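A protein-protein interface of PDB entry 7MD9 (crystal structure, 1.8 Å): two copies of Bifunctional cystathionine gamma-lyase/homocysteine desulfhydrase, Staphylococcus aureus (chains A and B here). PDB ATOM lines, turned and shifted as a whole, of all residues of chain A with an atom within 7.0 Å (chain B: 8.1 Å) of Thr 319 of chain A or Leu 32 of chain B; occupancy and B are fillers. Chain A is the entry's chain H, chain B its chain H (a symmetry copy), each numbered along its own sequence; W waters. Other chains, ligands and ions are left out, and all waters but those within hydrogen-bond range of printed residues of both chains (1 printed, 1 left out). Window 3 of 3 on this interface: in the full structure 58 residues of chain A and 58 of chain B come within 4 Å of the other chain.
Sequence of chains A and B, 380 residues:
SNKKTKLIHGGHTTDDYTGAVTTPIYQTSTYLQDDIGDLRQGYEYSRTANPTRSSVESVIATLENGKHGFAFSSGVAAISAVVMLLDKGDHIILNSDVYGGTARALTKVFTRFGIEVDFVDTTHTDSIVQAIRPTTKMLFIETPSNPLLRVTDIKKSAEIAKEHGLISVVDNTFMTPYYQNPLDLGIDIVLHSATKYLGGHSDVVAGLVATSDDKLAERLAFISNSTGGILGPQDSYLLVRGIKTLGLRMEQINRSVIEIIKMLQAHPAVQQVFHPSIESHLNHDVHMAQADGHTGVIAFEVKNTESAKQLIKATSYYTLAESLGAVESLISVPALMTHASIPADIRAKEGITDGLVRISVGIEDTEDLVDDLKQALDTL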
ATOM      1  N   ILE A 312      -6.794  -4.995  26.146  1.00  0.00           N
ATOM      2  CA  ILE A 312      -6.857  -6.214  25.346  1.00  0.00           C
ATOM      3  C   ILE A 312      -5.747  -6.232  24.304  1.00  0.00           C
ATOM      4  O   ILE A 312      -5.066  -7.248  24.115  1.00  0.00           O
ATOM      5  CB  ILE A 312      -8.244  -6.345  24.693  1.00  0.00           C
ATOM      6  CG1 ILE A 312      -9.298  -6.616  25.762  1.00  0.00           C
ATOM      7  CG2 ILE A 312      -8.234  -7.434  23.621  1.00  0.00           C
ATOM      8  CD1 ILE A 312     -10.721  -6.374  25.287  1.00  0.00           C
ATOM      9  N   THR A 315      -2.111  -6.957  25.808  1.00  0.00           N
ATOM     10  CA  THR A 315      -1.762  -8.246  26.394  1.00  0.00           C
ATOM     11  C   THR A 315      -1.179  -9.179  25.342  1.00  0.00           C
ATOM     12  O   THR A 315      -1.507  -9.096  24.154  1.00  0.00           O
ATOM     13  CB  THR A 315      -2.985  -8.912  27.035  1.00  0.00           C
ATOM     14  OG1 THR A 315      -4.078  -8.917  26.106  1.00  0.00           O
ATOM     15  CG2 THR A 315      -3.396  -8.179  28.300  1.00  0.00           C
ATOM     16  N   SER A 316      -0.294 -10.069  25.789  1.00  0.00           N
ATOM     17  CA  SER A 316       0.233 -11.112  24.924  1.00  0.00           C
ATOM     18  C   SER A 316      -0.441 -12.458  25.130  1.00  0.00           C
ATOM     19  O   SER A 316      -0.543 -13.239  24.178  1.00  0.00           O
ATOM     20  CB  SER A 316       1.744 -11.283  25.142  1.00  0.00           C
ATOM     21  OG  SER A 316       2.460 -10.153  24.676  1.00  0.00           O
ATOM     22  N   TYR A 317      -0.909 -12.744  26.344  1.00  0.00           N
ATOM     23  CA  TYR A 317      -1.378 -14.078  26.698  1.00  0.00           C
ATOM     24  C   TYR A 317      -2.862 -14.126  27.027  1.00  0.00           C
ATOM     25  O   TYR A 317      -3.342 -15.163  27.497  1.00  0.00           O
ATOM     26  CB  TYR A 317      -0.576 -14.616  27.881  1.00  0.00           C
ATOM     27  CG  TYR A 317       0.907 -14.576  27.623  1.00  0.00           C
ATOM     28  CD1 TYR A 317       1.429 -15.051  26.429  1.00  0.00           C
ATOM     29  CD2 TYR A 317       1.783 -14.045  28.559  1.00  0.00           C
ATOM     30  CE1 TYR A 317       2.793 -15.012  26.176  1.00  0.00           C
ATOM     31  CE2 TYR A 317       3.140 -13.999  28.317  1.00  0.00           C
ATOM     32  CZ  TYR A 317       3.639 -14.484  27.122  1.00  0.00           C
ATOM     33  OH  TYR A 317       4.990 -14.444  26.867  1.00  0.00           O
ATOM     34  N   TYR A 318      -3.598 -13.042  26.808  1.00  0.00           N
ATOM     35  CA  TYR A 318      -5.041 -13.037  26.993  1.00  0.00           C
ATOM     36  C   TYR A 318      -5.707 -12.927  25.634  1.00  0.00           C
ATOM     37  O   TYR A 318      -5.415 -12.004  24.866  1.00  0.00           O
ATOM     38  CB  TYR A 318      -5.484 -11.893  27.903  1.00  0.00           C
ATOM     39  CG  TYR A 318      -4.997 -12.042  29.321  1.00  0.00           C
ATOM     40  CD1 TYR A 318      -3.674 -11.768  29.651  1.00  0.00           C
ATOM     41  CD2 TYR A 318      -5.853 -12.464  30.328  1.00  0.00           C
ATOM     42  CE1 TYR A 318      -3.227 -11.897  30.951  1.00  0.00           C
ATOM     43  CE2 TYR A 318      -5.416 -12.596  31.625  1.00  0.00           C
ATOM     44  CZ  TYR A 318      -4.093 -12.321  31.928  1.00  0.00           C
ATOM     45  OH  TYR A 318      -3.656 -12.450  33.224  1.00  0.00           O
ATOM     46  N   THR A 319      -6.602 -13.863  25.346  1.00  0.00           N
ATOM     47  CA  THR A 319      -7.184 -14.016  24.022  1.00  0.00           C
ATOM     48  C   THR A 319      -8.601 -13.453  24.008  1.00  0.00           C
ATOM     49  O   THR A 319      -9.415 -13.792  24.871  1.00  0.00           O
ATOM     50  CB  THR A 319      -7.190 -15.490  23.629  1.00  0.00           C
ATOM     51  OG1 THR A 319      -5.842 -15.918  23.366  1.00  0.00           O
ATOM     52  CG2 THR A 319      -8.057 -15.706  22.412  1.00  0.00           C
ATOM     53  N   LEU A 320      -8.888 -12.588  23.032  1.00  0.00           N
ATOM     54  CA  LEU A 320     -10.220 -12.004  22.886  1.00  0.00           C
ATOM     55  C   LEU A 320     -11.119 -13.000  22.165  1.00  0.00           C
ATOM     56  O   LEU A 320     -10.960 -13.238  20.960  1.00  0.00           O
ATOM     57  CB  LEU A 320     -10.150 -10.683  22.122  1.00  0.00           C
ATOM     58  CG  LEU A 320     -11.506 -10.054  21.790  1.00  0.00           C
ATOM     59  CD1 LEU A 320     -12.239  -9.678  23.073  1.00  0.00           C
ATOM     60  CD2 LEU A 320     -11.337  -8.843  20.871  1.00  0.00           C
ATOM     61  N   ALA A 321     -12.066 -13.575  22.897  1.00  0.00           N
ATOM     62  CA  ALA A 321     -12.976 -14.566  22.338  1.00  0.00           C
ATOM     63  C   ALA A 321     -14.113 -14.784  23.324  1.00  0.00           C
ATOM     64  O   ALA A 321     -14.009 -14.436  24.502  1.00  0.00           O
ATOM     65  CB  ALA A 321     -12.260 -15.890  22.040  1.00  0.00           C
ATOM     66  N   GLU A 322     -15.196 -15.367  22.824  1.00  0.00           N
ATOM     67  CA  GLU A 322     -16.364 -15.745  23.667  1.00  0.00           C
ATOM     68  C   GLU A 322     -16.022 -17.009  24.466  1.00  0.00           C
ATOM     69  O   GLU A 322     -14.940 -17.585  24.229  1.00  0.00           O
ATOM     70  CB  GLU A 322     -17.606 -15.962  22.799  1.00  0.00           C
ATOM     71  CG  GLU A 322     -18.164 -14.682  22.198  1.00  0.00           C
ATOM     72  CD  GLU A 322     -18.848 -13.743  23.179  1.00  0.00           C
ATOM     73  OE1 GLU A 322     -19.061 -14.146  24.341  1.00  0.00           O
ATOM     74  OE2 GLU A 322     -19.170 -12.608  22.777  1.00  0.00           O
ATOM     75  N   GLU A 328      -6.521 -21.645  27.350  1.00  0.00           N
ATOM     76  CA  GLU A 328      -6.060 -20.274  27.147  1.00  0.00           C
ATOM     77  C   GLU A 328      -6.796 -19.321  28.074  1.00  0.00           C
ATOM     78  O   GLU A 328      -7.992 -19.484  28.328  1.00  0.00           O
ATOM     79  CB  GLU A 328      -6.306 -19.807  25.710  1.00  0.00           C
ATOM     80  CG  GLU A 328      -5.595 -20.576  24.633  1.00  0.00           C
ATOM     81  CD  GLU A 328      -6.373 -21.786  24.175  1.00  0.00           C
ATOM     82  OE1 GLU A 328      -7.507 -21.994  24.673  1.00  0.00           O
ATOM     83  OE2 GLU A 328      -5.843 -22.537  23.326  1.00  0.00           O
ATOM     84  N   SER A 329      -6.094 -18.300  28.552  1.00  0.00           N
ATOM     85  CA  SER A 329      -6.775 -17.222  29.251  1.00  0.00           C
ATOM     86  C   SER A 329      -7.550 -16.373  28.245  1.00  0.00           C
ATOM     87  O   SER A 329      -7.027 -16.002  27.191  1.00  0.00           O
ATOM     88  CB  SER A 329      -5.774 -16.373  30.030  1.00  0.00           C
ATOM     89  OG  SER A 329      -5.254 -17.099  31.137  1.00  0.00           O
ATOM     90  N   LEU A 330      -8.813 -16.099  28.555  1.00  0.00           N
ATOM     91  CA  LEU A 330      -9.685 -15.375  27.649  1.00  0.00           C
ATOM     92  C   LEU A 330     -10.062 -14.037  28.270  1.00  0.00           C
ATOM     93  O   LEU A 330     -10.174 -13.910  29.491  1.00  0.00           O
ATOM     94  CB  LEU A 330     -10.952 -16.177  27.337  1.00  0.00           C
ATOM     95  CG  LEU A 330     -10.727 -17.551  26.707  1.00  0.00           C
ATOM     96  CD1 LEU A 330     -12.068 -18.220  26.431  1.00  0.00           C
ATOM     97  CD2 LEU A 330      -9.912 -17.432  25.428  1.00  0.00           C
ATOM     98  N   ILE A 331     -10.271 -13.042  27.421  1.00  0.00           N
ATOM     99  CA  ILE A 331     -10.618 -11.709  27.898  1.00  0.00           C
ATOM    100  C   ILE A 331     -11.784 -11.186  27.075  1.00  0.00           C
ATOM    101  O   ILE A 331     -11.917 -11.496  25.888  1.00  0.00           O
ATOM    102  CB  ILE A 331      -9.390 -10.769  27.828  1.00  0.00           C
ATOM    103  CG1 ILE A 331      -9.677  -9.409  28.477  1.00  0.00           C
ATOM    104  CG2 ILE A 331      -8.880 -10.657  26.389  1.00  0.00           C
ATOM    105  CD1 ILE A 331      -8.427  -8.721  29.000  1.00  0.00           C
ATOM    106  N   SER A 332     -12.646 -10.405  27.721  1.00  0.00           N
ATOM    107  CA  SER A 332     -13.873  -9.930  27.090  1.00  0.00           C
ATOM    108  C   SER A 332     -14.325  -8.653  27.787  1.00  0.00           C
ATOM    109  O   SER A 332     -13.885  -8.337  28.894  1.00  0.00           O
ATOM    110  CB  SER A 332     -14.981 -10.984  27.159  1.00  0.00           C
ATOM    111  OG  SER A 332     -15.408 -11.142  28.501  1.00  0.00           O
ATOM    112  N   GLU A 364      -1.890 -21.057  31.686  1.00  0.00           N
ATOM    113  CA  GLU A 364      -0.550 -20.547  31.425  1.00  0.00           C
ATOM    114  C   GLU A 364       0.207 -20.360  32.742  1.00  0.00           C
ATOM    115  O   GLU A 364      -0.364 -20.418  33.828  1.00  0.00           O
ATOM    116  CB  GLU A 364      -0.618 -19.219  30.665  1.00  0.00           C
ATOM    117  CG  GLU A 364      -1.276 -19.313  29.298  1.00  0.00           C
ATOM    118  CD  GLU A 364      -2.744 -18.889  29.329  1.00  0.00           C
ATOM    119  OE1 GLU A 364      -3.380 -19.042  30.392  1.00  0.00           O
ATOM    120  OE2 GLU A 364      -3.254 -18.410  28.290  1.00  0.00           O
ATOM    121  N   THR B  28     -14.308 -27.274  17.694  1.00  0.00           N
ATOM    122  CA  THR B  28     -13.946 -26.025  18.343  1.00  0.00           C
ATOM    123  C   THR B  28     -15.215 -25.416  18.914  1.00  0.00           C
ATOM    124  O   THR B  28     -16.309 -25.643  18.391  1.00  0.00           O
ATOM    125  CB  THR B  28     -13.265 -25.048  17.361  1.00  0.00           C
ATOM    126  OG1 THR B  28     -12.528 -24.068  18.102  1.00  0.00           O
ATOM    127  CG2 THR B  28     -14.301 -24.313  16.487  1.00  0.00           C
ATOM    128  N   THR B  30     -15.131 -21.871  20.106  1.00  0.00           N
ATOM    129  CA  THR B  30     -15.108 -20.415  20.058  1.00  0.00           C
ATOM    130  C   THR B  30     -14.023 -19.958  19.087  1.00  0.00           C
ATOM    131  O   THR B  30     -13.235 -20.761  18.578  1.00  0.00           O
ATOM    132  CB  THR B  30     -14.935 -19.829  21.465  1.00  0.00           C
ATOM    133  OG1 THR B  30     -15.099 -18.406  21.425  1.00  0.00           O
ATOM    134  CG2 THR B  30     -13.573 -20.177  22.021  1.00  0.00           C
ATOM    135  N   TYR B  31     -14.026 -18.655  18.785  1.00  0.00           N
ATOM    136  CA  TYR B  31     -13.234 -18.129  17.678  1.00  0.00           C
ATOM    137  C   TYR B  31     -12.590 -16.806  18.073  1.00  0.00           C
ATOM    138  O   TYR B  31     -13.223 -15.964  18.717  1.00  0.00           O
ATOM    139  CB  TYR B  31     -14.098 -17.947  16.407  1.00  0.00           C
ATOM    140  CG  TYR B  31     -14.870 -19.198  16.023  1.00  0.00           C
ATOM    141  CD1 TYR B  31     -16.017 -19.570  16.723  1.00  0.00           C
ATOM    142  CD2 TYR B  31     -14.442 -20.011  14.979  1.00  0.00           C
ATOM    143  CE1 TYR B  31     -16.709 -20.718  16.408  1.00  0.00           C
ATOM    144  CE2 TYR B  31     -15.138 -21.175  14.649  1.00  0.00           C
ATOM    145  CZ  TYR B  31     -16.273 -21.514  15.374  1.00  0.00           C
ATOM    146  OH  TYR B  31     -16.975 -22.657  15.078  1.00  0.00           O
ATOM    147  N   LEU B  32     -11.322 -16.634  17.686  1.00  0.00           N
ATOM    148  CA  LEU B  32     -10.642 -15.361  17.911  1.00  0.00           C
ATOM    149  C   LEU B  32     -11.377 -14.224  17.215  1.00  0.00           C
ATOM    150  O   LEU B  32     -11.827 -14.359  16.073  1.00  0.00           O
ATOM    151  CB  LEU B  32      -9.201 -15.417  17.397  1.00  0.00           C
ATOM    152  CG  LEU B  32      -8.369 -16.615  17.848  1.00  0.00           C
ATOM    153  CD1 LEU B  32      -7.379 -17.083  16.777  1.00  0.00           C
ATOM    154  CD2 LEU B  32      -7.643 -16.253  19.108  1.00  0.00           C
ATOM    155  N   GLN B  33     -11.487 -13.094  17.908  1.00  0.00           N
ATOM    156  CA  GLN B  33     -11.937 -11.844  17.312  1.00  0.00           C
ATOM    157  C   GLN B  33     -10.749 -10.889  17.241  1.00  0.00           C
ATOM    158  O   GLN B  33     -10.055 -10.682  18.241  1.00  0.00           O
ATOM    159  CB  GLN B  33     -13.078 -11.229  18.121  1.00  0.00           C
ATOM    160  CG  GLN B  33     -14.299 -12.149  18.267  1.00  0.00           C
ATOM    161  CD  GLN B  33     -15.403 -11.531  19.099  1.00  0.00           C
ATOM    162  OE1 GLN B  33     -15.540 -10.308  19.150  1.00  0.00           O
ATOM    163  NE2 GLN B  33     -16.200 -12.373  19.764  1.00  0.00           N
ATOM    164  N   ASP B  34     -10.499 -10.333  16.055  1.00  0.00           N
ATOM    165  CA  ASP B  34      -9.356  -9.435  15.906  1.00  0.00           C
ATOM    166  C   ASP B  34      -9.618  -8.088  16.568  1.00  0.00           C
ATOM    167  O   ASP B  34      -8.696  -7.469  17.110  1.00  0.00           O
ATOM    168  CB  ASP B  34      -9.022  -9.275  14.425  1.00  0.00           C
ATOM    169  CG  ASP B  34      -8.496 -10.568  13.812  1.00  0.00           C
ATOM    170  OD1 ASP B  34      -7.739 -11.278  14.508  1.00  0.00           O
ATOM    171  OD2 ASP B  34      -8.854 -10.884  12.658  1.00  0.00           O
ATOM    172  N   ASP B  35     -10.861  -7.631  16.540  1.00  0.00           N
ATOM    173  CA  ASP B  35     -11.338  -6.508  17.330  1.00  0.00           C
ATOM    174  C   ASP B  35     -12.688  -6.910  17.892  1.00  0.00           C
ATOM    175  O   ASP B  35     -13.342  -7.812  17.366  1.00  0.00           O
ATOM    176  CB  ASP B  35     -11.480  -5.223  16.501  1.00  0.00           C
ATOM    177  CG  ASP B  35     -10.159  -4.742  15.938  1.00  0.00           C
ATOM    178  OD1 ASP B  35      -9.423  -4.038  16.663  1.00  0.00           O
ATOM    179  OD2 ASP B  35      -9.858  -5.072  14.769  1.00  0.00           O
ATOM    180  N   ASP B  38     -15.678  -7.899  15.622  1.00  0.00           N
ATOM    181  CA  ASP B  38     -15.270  -8.163  14.250  1.00  0.00           C
ATOM    182  C   ASP B  38     -14.893  -9.633  14.134  1.00  0.00           C
ATOM    183  O   ASP B  38     -13.870 -10.068  14.674  1.00  0.00           O
ATOM    184  CB  ASP B  38     -14.119  -7.251  13.833  1.00  0.00           C
ATOM    185  CG  ASP B  38     -14.552  -5.801  13.694  1.00  0.00           C
ATOM    186  OD1 ASP B  38     -15.753  -5.515  13.907  1.00  0.00           O
ATOM    187  OD2 ASP B  38     -13.698  -4.951  13.353  1.00  0.00           O
ATOM    188  N   LEU B  39     -15.727 -10.391  13.433  1.00  0.00           N
ATOM    189  CA  LEU B  39     -15.512 -11.811  13.205  1.00  0.00           C
ATOM    190  C   LEU B  39     -14.820 -11.992  11.864  1.00  0.00           C
ATOM    191  O   LEU B  39     -15.254 -11.418  10.862  1.00  0.00           O
ATOM    192  CB  LEU B  39     -16.847 -12.559  13.234  1.00  0.00           C
ATOM    193  CG  LEU B  39     -17.809 -12.125  14.348  1.00  0.00           C
ATOM    194  CD1 LEU B  39     -19.125 -12.911  14.308  1.00  0.00           C
ATOM    195  CD2 LEU B  39     -17.146 -12.261  15.716  1.00  0.00           C
ATOM    196  N   ARG B  40     -13.746 -12.785  11.848  1.00  0.00           N
ATOM    197  CA  ARG B  40     -12.980 -12.980  10.620  1.00  0.00           C
ATOM    198  C   ARG B  40     -13.847 -13.543   9.507  1.00  0.00           C
ATOM    199  O   ARG B  40     -13.758 -13.107   8.352  1.00  0.00           O
ATOM    200  CB  ARG B  40     -11.802 -13.927  10.868  1.00  0.00           C
ATOM    201  CG  ARG B  40     -10.946 -13.574  12.039  1.00  0.00           C
ATOM    202  CD  ARG B  40      -9.659 -14.373  11.995  1.00  0.00           C
ATOM    203  NE  ARG B  40      -8.667 -13.800  12.892  1.00  0.00           N
ATOM    204  CZ  ARG B  40      -7.618 -14.459  13.365  1.00  0.00           C
ATOM    205  NH1 ARG B  40      -7.424 -15.729  13.028  1.00  0.00           N
ATOM    206  NH2 ARG B  40      -6.766 -13.846  14.176  1.00  0.00           N
ATOM    207  N   GLN B  41     -14.657 -14.554   9.823  1.00  0.00           N
ATOM    208  CA  GLN B  41     -15.473 -15.229   8.820  1.00  0.00           C
ATOM    209  C   GLN B  41     -16.901 -15.430   9.302  1.00  0.00           C
ATOM    210  O   GLN B  41     -17.596 -16.325   8.804  1.00  0.00           O
ATOM    211  CB  GLN B  41     -14.857 -16.575   8.426  1.00  0.00           C
ATOM    212  CG  GLN B  41     -13.554 -16.455   7.678  1.00  0.00           C
ATOM    213  CD  GLN B  41     -13.717 -15.798   6.326  1.00  0.00           C
ATOM    214  OE1 GLN B  41     -14.763 -15.918   5.685  1.00  0.00           O
ATOM    215  NE2 GLN B  41     -12.678 -15.100   5.879  1.00  0.00           N
ATOM    216  N   GLY B  42     -17.345 -14.624  10.265  1.00  0.00           N
ATOM    217  CA  GLY B  42     -18.709 -14.665  10.736  1.00  0.00           C
ATOM    218  C   GLY B  42     -18.969 -15.629  11.869  1.00  0.00           C
ATOM    219  O   GLY B  42     -20.130 -15.784  12.269  1.00  0.00           O
ATOM    220  N   TYR B  43     -17.935 -16.276  12.399  1.00  0.00           N
ATOM    221  CA  TYR B  43     -18.080 -17.238  13.481  1.00  0.00           C
ATOM    222  C   TYR B  43     -17.630 -16.609  14.789  1.00  0.00           C
ATOM    223  O   TYR B  43     -16.653 -15.857  14.827  1.00  0.00           O
ATOM    224  CB  TYR B  43     -17.280 -18.513  13.182  1.00  0.00           C
ATOM    225  CG  TYR B  43     -17.858 -19.238  11.992  1.00  0.00           C
ATOM    226  CD1 TYR B  43     -18.959 -20.076  12.138  1.00  0.00           C
ATOM    227  CD2 TYR B  43     -17.347 -19.044  10.718  1.00  0.00           C
ATOM    228  CE1 TYR B  43     -19.512 -20.717  11.051  1.00  0.00           C
ATOM    229  CE2 TYR B  43     -17.899 -19.681   9.624  1.00  0.00           C
ATOM    230  CZ  TYR B  43     -18.986 -20.510   9.801  1.00  0.00           C
ATOM    231  OH  TYR B  43     -19.548 -21.146   8.719  1.00  0.00           O
ATOM    232  N   GLU B  44     -18.361 -16.906  15.858  1.00  0.00           N
ATOM    233  CA  GLU B  44     -18.004 -16.397  17.175  1.00  0.00           C
ATOM    234  C   GLU B  44     -18.254 -17.378  18.301  1.00  0.00           C
ATOM    235  O   GLU B  44     -17.579 -17.275  19.331  1.00  0.00           O
ATOM    236  CB  GLU B  44     -18.752 -15.084  17.471  1.00  0.00           C
ATOM    237  CG  GLU B  44     -20.134 -15.222  18.042  1.00  0.00           C
ATOM    238  CD  GLU B  44     -20.865 -13.877  18.118  1.00  0.00           C
ATOM    239  OE1 GLU B  44     -21.800 -13.665  17.325  1.00  0.00           O
ATOM    240  OE2 GLU B  44     -20.503 -13.035  18.964  1.00  0.00           O
ATOM    241  N   TYR B  45     -19.162 -18.345  18.143  1.00  0.00           N
ATOM    242  CA  TYR B  45     -19.461 -19.327  19.181  1.00  0.00           C
ATOM    243  C   TYR B  45     -20.202 -20.489  18.532  1.00  0.00           C
ATOM    244  O   TYR B  45     -21.203 -20.270  17.847  1.00  0.00           O
ATOM    245  CB  TYR B  45     -20.307 -18.708  20.294  1.00  0.00           C
ATOM    246  CG  TYR B  45     -20.439 -19.566  21.529  1.00  0.00           C
ATOM    247  CD1 TYR B  45     -19.355 -19.767  22.369  1.00  0.00           C
ATOM    248  CD2 TYR B  45     -21.657 -20.160  21.866  1.00  0.00           C
ATOM    249  CE1 TYR B  45     -19.466 -20.538  23.514  1.00  0.00           C
ATOM    250  CE2 TYR B  45     -21.779 -20.935  23.016  1.00  0.00           C
ATOM    251  CZ  TYR B  45     -20.678 -21.116  23.839  1.00  0.00           C
ATOM    252  OH  TYR B  45     -20.767 -21.874  24.989  1.00  0.00           O
HETATM  253  O   HOH W   1     -15.664 -15.422  19.910  1.00  0.00           O
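The backbone carbonyl oxygen (O) of Glu 322 of chain A lies within hydrogen-bond range of the side-chain hydroxyl (OG1) of Thr 30 of chain B, 2.9 Å away.
The backbone carbonyl oxygen of Leu 320 of chain A lies within hydrogen-bond range of the backbone NH of Gln 33 of chain B (3.1 Å).
Thr 319 of chain A touches Leu 32 of chain B (CG2 to CD2, 3.4 Å).
Leu 32 of chain B touches Leu 320 of chain A.
Asp 35 of chain B touches Leu 320 of chain A.
CB of Ala 321 of chain A touches OG1 of Thr 30 of chain B, 3.8 Å away.
Ala 321 of chain A touches Tyr 31 of chain B (CB to O, 3.5 Å).
CG of Glu 322 of chain A touches NE2 of Gln 33 of chain B, at 3.9 Å.
Glu 44 of chain B touches Glu 322 of chain A (O to CB, 3.7 Å).
Water W1 lies within hydrogen-bond range of the backbone carbonyl oxygen (O) of Glu 44 of chain B (2.7 Å), the backbone carbonyl oxygen (O) of Tyr 31 of chain B (2.8 Å), the backbone NH (N) of Glu 322 of chain A (3.0 Å), the side-chain amide nitrogen (NE2) of Gln 33 of chain B (3.1 Å) and the side-chain hydroxyl (OG1) of Thr 30 of chain B (3.4 Å).
No position is printed for both chains.
Of the 9 pairs that touch across the chains among the printed residues, none has its exchanged pair printed and touching as well.
The backbone carbonyl oxygen of Thr 30 of chain B is in hydrogen-bond range of the side-chain hydroxyl of Thr 28 of chain B (3.4 Å).
The backbone NH (N) of Ile 331 of chain A sits at hydrogen-bond distance from the backbone carbonyl oxygen (O) of Thr 319 of chain A.
N of Thr 319 of chain A is in hydrogen-bond range of O of Ser 329 of chain A, at 2.9 Å.
O of Glu 44 of chain B lies within hydrogen-bond range of OG1 of Thr 30 of chain B (3.4 Å).
Thr 319 of chain A touches just one residue of chain B: Leu 32 (3.4 Å).
Of chain A, only Thr 319 and Leu 320 come within 4 Å of Leu 32 of chain B.
Printed residues of chain A within 4 Å of Asp 35 of chain B: Leu 320 (3.8 Å).
Of the printed residues of chain B, Glu 322 of chain A touches Thr 30, Gln 33 and Glu 44.
Of the printed residues of chain B, Ala 321 of chain A touches Thr 30 and Tyr 31.
Of the printed residues of chain A, Tyr 31 of chain B touches Ala 321 (3.5 Å).
Ser 316 of chain A touches none of the printed residues of chain B.
The nearest residue of chain A that does not touch Leu 32 of chain B is Ala 321 of chain A (4.5 Å).
Printed residues of chain B that touch a printed residue of chain A: Thr 30, Tyr 31, Leu 32, Gln 33, Asp 35 and Glu 44.
Hydrophobic or aromatic side chains of chain B that line the printed part of chain A: Leu 32.
Along chain B the printed residues that touch a printed residue of chain A span positions 30 to 44.
Of the 15 printed residues of chain A, 4 touch a printed residue of chain B.
Printed residues of chain A that touch a printed residue of chain B: Thr 319, Leu 320, Ala 321 and Glu 322.
Hydrophobic or aromatic side chains of chain A that line the printed part of chain B: Leu 320 and Ala 321.
Among the printed residues, no Asp or Glu carboxylate lies within 4 Å of a Lys or Arg side-chain nitrogen of the other chain.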
